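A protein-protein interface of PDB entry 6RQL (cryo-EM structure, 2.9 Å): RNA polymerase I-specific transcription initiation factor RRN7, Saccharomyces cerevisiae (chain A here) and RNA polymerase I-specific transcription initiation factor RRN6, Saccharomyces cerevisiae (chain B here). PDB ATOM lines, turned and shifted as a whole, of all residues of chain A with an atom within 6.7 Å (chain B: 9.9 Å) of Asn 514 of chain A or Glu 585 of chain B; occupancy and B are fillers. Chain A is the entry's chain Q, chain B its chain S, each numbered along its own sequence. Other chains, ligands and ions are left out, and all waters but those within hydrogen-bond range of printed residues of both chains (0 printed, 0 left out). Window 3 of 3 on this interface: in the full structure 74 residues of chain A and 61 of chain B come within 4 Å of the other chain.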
ATOM      1  N   PHE A 320      -7.669  15.712 -10.959  1.00  0.00           N
ATOM      2  CA  PHE A 320      -8.884  16.237 -11.573  1.00  0.00           C
ATOM      3  C   PHE A 320      -9.705  15.066 -12.096  1.00  0.00           C
ATOM      4  O   PHE A 320     -10.068  14.990 -13.267  1.00  0.00           O
ATOM      5  CB  PHE A 320      -8.511  17.229 -12.660  1.00  0.00           C
ATOM      6  CG  PHE A 320      -7.984  18.518 -12.119  1.00  0.00           C
ATOM      7  CD1 PHE A 320      -8.450  19.008 -10.904  1.00  0.00           C
ATOM      8  CD2 PHE A 320      -6.965  19.191 -12.757  1.00  0.00           C
ATOM      9  CE1 PHE A 320      -7.960  20.186 -10.378  1.00  0.00           C
ATOM     10  CE2 PHE A 320      -6.465  20.358 -12.223  1.00  0.00           C
ATOM     11  CZ  PHE A 320      -6.962  20.859 -11.040  1.00  0.00           C
ATOM     12  N   CYS A 509       3.826  24.365 -20.273  1.00  0.00           N
ATOM     13  CA  CYS A 509       2.570  23.804 -20.752  1.00  0.00           C
ATOM     14  C   CYS A 509       1.430  24.809 -20.648  1.00  0.00           C
ATOM     15  O   CYS A 509       0.503  24.774 -21.464  1.00  0.00           O
ATOM     16  CB  CYS A 509       2.228  22.528 -19.978  1.00  0.00           C
ATOM     17  SG  CYS A 509       0.786  21.621 -20.578  1.00  0.00           S
ATOM     18  N   LEU A 510       1.483  25.718 -19.674  1.00  0.00           N
ATOM     19  CA  LEU A 510       0.418  26.704 -19.553  1.00  0.00           C
ATOM     20  C   LEU A 510       0.748  27.989 -20.305  1.00  0.00           C
ATOM     21  O   LEU A 510      -0.166  28.684 -20.757  1.00  0.00           O
ATOM     22  CB  LEU A 510       0.134  26.980 -18.073  1.00  0.00           C
ATOM     23  CG  LEU A 510      -1.170  27.679 -17.670  1.00  0.00           C
ATOM     24  CD1 LEU A 510      -1.635  27.117 -16.340  1.00  0.00           C
ATOM     25  CD2 LEU A 510      -1.023  29.192 -17.563  1.00  0.00           C
ATOM     26  N   HIS A 511       2.037  28.320 -20.446  1.00  0.00           N
ATOM     27  CA  HIS A 511       2.447  29.426 -21.305  1.00  0.00           C
ATOM     28  C   HIS A 511       2.099  29.172 -22.762  1.00  0.00           C
ATOM     29  O   HIS A 511       1.796  30.122 -23.489  1.00  0.00           O
ATOM     30  CB  HIS A 511       3.950  29.667 -21.165  1.00  0.00           C
ATOM     31  CG  HIS A 511       4.462  30.829 -21.958  1.00  0.00           C
ATOM     32  ND1 HIS A 511       4.880  30.713 -23.267  1.00  0.00           N
ATOM     33  CD2 HIS A 511       4.634  32.130 -21.623  1.00  0.00           C
ATOM     34  CE1 HIS A 511       5.282  31.893 -23.706  1.00  0.00           C
ATOM     35  NE2 HIS A 511       5.141  32.770 -22.728  1.00  0.00           N
ATOM     36  N   ARG A 512       2.128  27.914 -23.194  1.00  0.00           N
ATOM     37  CA  ARG A 512       1.706  27.546 -24.536  1.00  0.00           C
ATOM     38  C   ARG A 512       0.198  27.351 -24.620  1.00  0.00           C
ATOM     39  O   ARG A 512      -0.392  27.589 -25.680  1.00  0.00           O
ATOM     40  CB  ARG A 512       2.439  26.275 -24.983  1.00  0.00           C
ATOM     41  CG  ARG A 512       2.230  25.890 -26.439  1.00  0.00           C
ATOM     42  CD  ARG A 512       3.079  24.702 -26.842  1.00  0.00           C
ATOM     43  NE  ARG A 512       2.887  24.357 -28.245  1.00  0.00           N
ATOM     44  CZ  ARG A 512       1.981  23.488 -28.678  1.00  0.00           C
ATOM     45  NH1 ARG A 512       1.187  22.869 -27.816  1.00  0.00           N
ATOM     46  NH2 ARG A 512       1.870  23.234 -29.973  1.00  0.00           N
ATOM     47  N   MET A 513      -0.447  26.961 -23.519  1.00  0.00           N
ATOM     48  CA  MET A 513      -1.900  26.836 -23.544  1.00  0.00           C
ATOM     49  C   MET A 513      -2.582  28.197 -23.593  1.00  0.00           C
ATOM     50  O   MET A 513      -3.268  28.521 -24.570  1.00  0.00           O
ATOM     51  CB  MET A 513      -2.403  26.063 -22.330  1.00  0.00           C
ATOM     52  CG  MET A 513      -3.903  25.902 -22.378  1.00  0.00           C
ATOM     53  SD  MET A 513      -4.632  24.984 -21.027  1.00  0.00           S
ATOM     54  CE  MET A 513      -6.349  25.077 -21.527  1.00  0.00           C
ATOM     55  N   ASN A 514      -2.405  29.008 -22.555  1.00  0.00           N
ATOM     56  CA  ASN A 514      -3.032  30.324 -22.509  1.00  0.00           C
ATOM     57  C   ASN A 514      -2.218  31.345 -23.296  1.00  0.00           C
ATOM     58  O   ASN A 514      -2.147  31.281 -24.524  1.00  0.00           O
ATOM     59  CB  ASN A 514      -3.206  30.787 -21.062  1.00  0.00           C
ATOM     60  CG  ASN A 514      -4.224  29.960 -20.302  1.00  0.00           C
ATOM     61  OD1 ASN A 514      -3.885  29.245 -19.359  1.00  0.00           O
ATOM     62  ND2 ASN A 514      -5.485  30.068 -20.701  1.00  0.00           N
ATOM     63  N   ASN B 579      -0.678  22.690  -7.538  1.00  0.00           N
ATOM     64  CA  ASN B 579      -1.944  23.047  -6.897  1.00  0.00           C
ATOM     65  C   ASN B 579      -1.994  24.535  -6.535  1.00  0.00           C
ATOM     66  O   ASN B 579      -2.135  24.927  -5.375  1.00  0.00           O
ATOM     67  CB  ASN B 579      -2.159  22.156  -5.670  1.00  0.00           C
ATOM     68  CG  ASN B 579      -2.177  20.688  -6.029  1.00  0.00           C
ATOM     69  OD1 ASN B 579      -2.816  20.283  -6.997  1.00  0.00           O
ATOM     70  ND2 ASN B 579      -1.437  19.887  -5.278  1.00  0.00           N
ATOM     71  N   ASN B 580      -1.871  25.356  -7.574  1.00  0.00           N
ATOM     72  CA  ASN B 580      -1.975  26.795  -7.402  1.00  0.00           C
ATOM     73  C   ASN B 580      -3.448  27.201  -7.307  1.00  0.00           C
ATOM     74  O   ASN B 580      -4.352  26.474  -7.728  1.00  0.00           O
ATOM     75  CB  ASN B 580      -1.262  27.512  -8.548  1.00  0.00           C
ATOM     76  CG  ASN B 580       0.216  27.166  -8.619  1.00  0.00           C
ATOM     77  OD1 ASN B 580       0.670  26.545  -9.577  1.00  0.00           O
ATOM     78  ND2 ASN B 580       0.970  27.560  -7.603  1.00  0.00           N
ATOM     79  N   ALA B 581      -3.692  28.387  -6.752  1.00  0.00           N
ATOM     80  CA  ALA B 581      -5.046  28.853  -6.450  1.00  0.00           C
ATOM     81  C   ALA B 581      -5.594  29.780  -7.527  1.00  0.00           C
ATOM     82  O   ALA B 581      -6.330  30.727  -7.230  1.00  0.00           O
ATOM     83  CB  ALA B 581      -5.078  29.539  -5.090  1.00  0.00           C
ATOM     84  N   ASP B 582      -5.254  29.519  -8.789  1.00  0.00           N
ATOM     85  CA  ASP B 582      -5.739  30.308  -9.915  1.00  0.00           C
ATOM     86  C   ASP B 582      -7.129  29.812 -10.299  1.00  0.00           C
ATOM     87  O   ASP B 582      -7.276  28.698 -10.812  1.00  0.00           O
ATOM     88  CB  ASP B 582      -4.777  30.205 -11.096  1.00  0.00           C
ATOM     89  CG  ASP B 582      -3.451  30.897 -10.832  1.00  0.00           C
ATOM     90  OD1 ASP B 582      -3.434  31.868 -10.053  1.00  0.00           O
ATOM     91  OD2 ASP B 582      -2.426  30.472 -11.404  1.00  0.00           O
ATOM     92  N   GLU B 583      -8.150  30.635 -10.043  1.00  0.00           N
ATOM     93  CA  GLU B 583      -9.495  30.312 -10.508  1.00  0.00           C
ATOM     94  C   GLU B 583      -9.600  30.425 -12.021  1.00  0.00           C
ATOM     95  O   GLU B 583     -10.426  29.741 -12.636  1.00  0.00           O
ATOM     96  CB  GLU B 583     -10.538  31.234  -9.867  1.00  0.00           C
ATOM     97  CG  GLU B 583     -10.701  31.104  -8.362  1.00  0.00           C
ATOM     98  CD  GLU B 583      -9.771  32.017  -7.594  1.00  0.00           C
ATOM     99  OE1 GLU B 583      -9.052  32.809  -8.236  1.00  0.00           O
ATOM    100  OE2 GLU B 583      -9.763  31.950  -6.350  1.00  0.00           O
ATOM    101  N   ARG B 584      -8.787  31.294 -12.623  1.00  0.00           N
ATOM    102  CA  ARG B 584      -8.732  31.390 -14.075  1.00  0.00           C
ATOM    103  C   ARG B 584      -8.146  30.122 -14.677  1.00  0.00           C
ATOM    104  O   ARG B 584      -8.693  29.563 -15.635  1.00  0.00           O
ATOM    105  CB  ARG B 584      -7.911  32.617 -14.480  1.00  0.00           C
ATOM    106  CG  ARG B 584      -7.797  32.824 -15.971  1.00  0.00           C
ATOM    107  CD  ARG B 584      -9.163  33.121 -16.562  1.00  0.00           C
ATOM    108  NE  ARG B 584      -9.117  33.302 -18.008  1.00  0.00           N
ATOM    109  CZ  ARG B 584      -9.172  32.305 -18.884  1.00  0.00           C
ATOM    110  NH1 ARG B 584      -9.263  31.051 -18.460  1.00  0.00           N
ATOM    111  NH2 ARG B 584      -9.125  32.561 -20.183  1.00  0.00           N
ATOM    112  N   GLU B 585      -7.043  29.639 -14.109  1.00  0.00           N
ATOM    113  CA  GLU B 585      -6.357  28.455 -14.603  1.00  0.00           C
ATOM    114  C   GLU B 585      -6.693  27.205 -13.795  1.00  0.00           C
ATOM    115  O   GLU B 585      -5.877  26.281 -13.713  1.00  0.00           O
ATOM    116  CB  GLU B 585      -4.846  28.695 -14.631  1.00  0.00           C
ATOM    117  CG  GLU B 585      -4.383  29.661 -15.726  1.00  0.00           C
ATOM    118  CD  GLU B 585      -4.473  31.128 -15.332  1.00  0.00           C
ATOM    119  OE1 GLU B 585      -4.811  31.424 -14.168  1.00  0.00           O
ATOM    120  OE2 GLU B 585      -4.212  31.989 -16.198  1.00  0.00           O
ATOM    121  N   LYS B 586      -7.878  27.156 -13.188  1.00  0.00           N
ATOM    122  CA  LYS B 586      -8.312  25.920 -12.548  1.00  0.00           C
ATOM    123  C   LYS B 586      -8.753  24.900 -13.585  1.00  0.00           C
ATOM    124  O   LYS B 586      -8.198  23.800 -13.667  1.00  0.00           O
ATOM    125  CB  LYS B 586      -9.454  26.184 -11.568  1.00  0.00           C
ATOM    126  CG  LYS B 586      -9.923  24.897 -10.906  1.00  0.00           C
ATOM    127  CD  LYS B 586     -11.048  25.093  -9.910  1.00  0.00           C
ATOM    128  CE  LYS B 586     -11.469  23.742  -9.340  1.00  0.00           C
ATOM    129  NZ  LYS B 586     -12.573  23.840  -8.354  1.00  0.00           N
ATOM    130  N   GLU B 587      -9.746  25.257 -14.390  1.00  0.00           N
ATOM    131  CA  GLU B 587     -10.279  24.392 -15.429  1.00  0.00           C
ATOM    132  C   GLU B 587      -9.364  24.320 -16.640  1.00  0.00           C
ATOM    133  O   GLU B 587      -9.586  23.479 -17.517  1.00  0.00           O
ATOM    134  CB  GLU B 587     -11.659  24.900 -15.862  1.00  0.00           C
ATOM    135  CG  GLU B 587     -11.603  26.098 -16.815  1.00  0.00           C
ATOM    136  CD  GLU B 587     -11.411  27.443 -16.131  1.00  0.00           C
ATOM    137  OE1 GLU B 587     -11.090  27.490 -14.925  1.00  0.00           O
ATOM    138  OE2 GLU B 587     -11.558  28.471 -16.824  1.00  0.00           O
ATOM    139  N   SER B 588      -8.361  25.203 -16.708  1.00  0.00           N
ATOM    140  CA  SER B 588      -7.371  25.162 -17.777  1.00  0.00           C
ATOM    141  C   SER B 588      -6.557  23.880 -17.715  1.00  0.00           C
ATOM    142  O   SER B 588      -6.199  23.311 -18.752  1.00  0.00           O
ATOM    143  CB  SER B 588      -6.462  26.385 -17.680  1.00  0.00           C
ATOM    144  OG  SER B 588      -5.412  26.333 -18.625  1.00  0.00           O
ATOM    145  N   ILE B 589      -6.271  23.401 -16.509  1.00  0.00           N
ATOM    146  CA  ILE B 589      -5.615  22.108 -16.391  1.00  0.00           C
ATOM    147  C   ILE B 589      -6.605  20.988 -16.691  1.00  0.00           C
ATOM    148  O   ILE B 589      -6.267  20.005 -17.358  1.00  0.00           O
ATOM    149  CB  ILE B 589      -4.989  21.967 -14.998  1.00  0.00           C
ATOM    150  CG1 ILE B 589      -4.071  23.148 -14.703  1.00  0.00           C
ATOM    151  CG2 ILE B 589      -4.172  20.705 -14.922  1.00  0.00           C
ATOM    152  CD1 ILE B 589      -3.619  23.199 -13.269  1.00  0.00           C
ATOM    153  N   GLY B 590      -7.853  21.142 -16.237  1.00  0.00           N
ATOM    154  CA  GLY B 590      -8.903  20.195 -16.566  1.00  0.00           C
ATOM    155  C   GLY B 590      -9.324  20.217 -18.021  1.00  0.00           C
ATOM    156  O   GLY B 590      -9.944  19.257 -18.490  1.00  0.00           O
ATOM    157  N   ALA B 591      -9.021  21.299 -18.740  1.00  0.00           N
ATOM    158  CA  ALA B 591      -9.337  21.346 -20.160  1.00  0.00           C
ATOM    159  C   ALA B 591      -8.500  20.355 -20.951  1.00  0.00           C
ATOM    160  O   ALA B 591      -9.014  19.707 -21.871  1.00  0.00           O
ATOM    161  CB  ALA B 591      -9.132  22.758 -20.705  1.00  0.00           C
ATOM    162  N   LEU B 592      -7.220  20.212 -20.610  1.00  0.00           N
ATOM    163  CA  LEU B 592      -6.393  19.244 -21.318  1.00  0.00           C
ATOM    164  C   LEU B 592      -6.673  17.834 -20.809  1.00  0.00           C
ATOM    165  O   LEU B 592      -6.455  16.854 -21.530  1.00  0.00           O
ATOM    166  CB  LEU B 592      -4.921  19.629 -21.169  1.00  0.00           C
ATOM    167  CG  LEU B 592      -3.897  19.212 -22.226  1.00  0.00           C
ATOM    168  CD1 LEU B 592      -2.793  20.248 -22.246  1.00  0.00           C
ATOM    169  CD2 LEU B 592      -3.314  17.827 -22.004  1.00  0.00           C
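Of the 14 printed residues of chain B, 4 touch a printed residue of chain A. Along chain B the printed residues that touch a printed residue of chain A span positions 585 to 591. Among the printed residues, no Asp or Glu carboxylate lies within 4 Å of a Lys or Arg side-chain nitrogen of the other chain.
CE2 of Phe 320 of chain A touches CB of Ile 589 of chain B, 3.5 Å away. CG of Glu 585 of chain B touches CD1 of Leu 510 of chain A (3.8 Å). Ala 591 of chain B touches Met 513 of chain A. Asn 514 of chain A touches Glu 585 of chain B.
The side-chain hydroxyl (OG) of Ser 588 of chain B lies within hydrogen-bond range of the side-chain sulfur (SD) of Met 513 of chain A (2.9 Å). OD1 of Asn 514 of chain A is in hydrogen-bond range of OG of Ser 588 of chain B (3.4 Å).
Of the printed residues of chain B, Phe 320 of chain A touches Ile 589 (3.5 Å). Printed residues of chain B within 4 Å of Leu 510 of chain A: Glu 585. Printed residues of chain B within 4 Å of Met 513 of chain A: Ser 588 and Ala 591. Of chain B, only Glu 585 (3.7 Å) and Ser 588 (3.4 Å) come within 4 Å of Asn 514 of chain A. Of chain A, only Leu 510 (3.8 Å) and Asn 514 (3.7 Å) come within 4 Å of Glu 585 of chain B. The nearest residue of chain B that does not touch Asn 514 of chain A is Arg 584 of chain B (4.4 Å).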
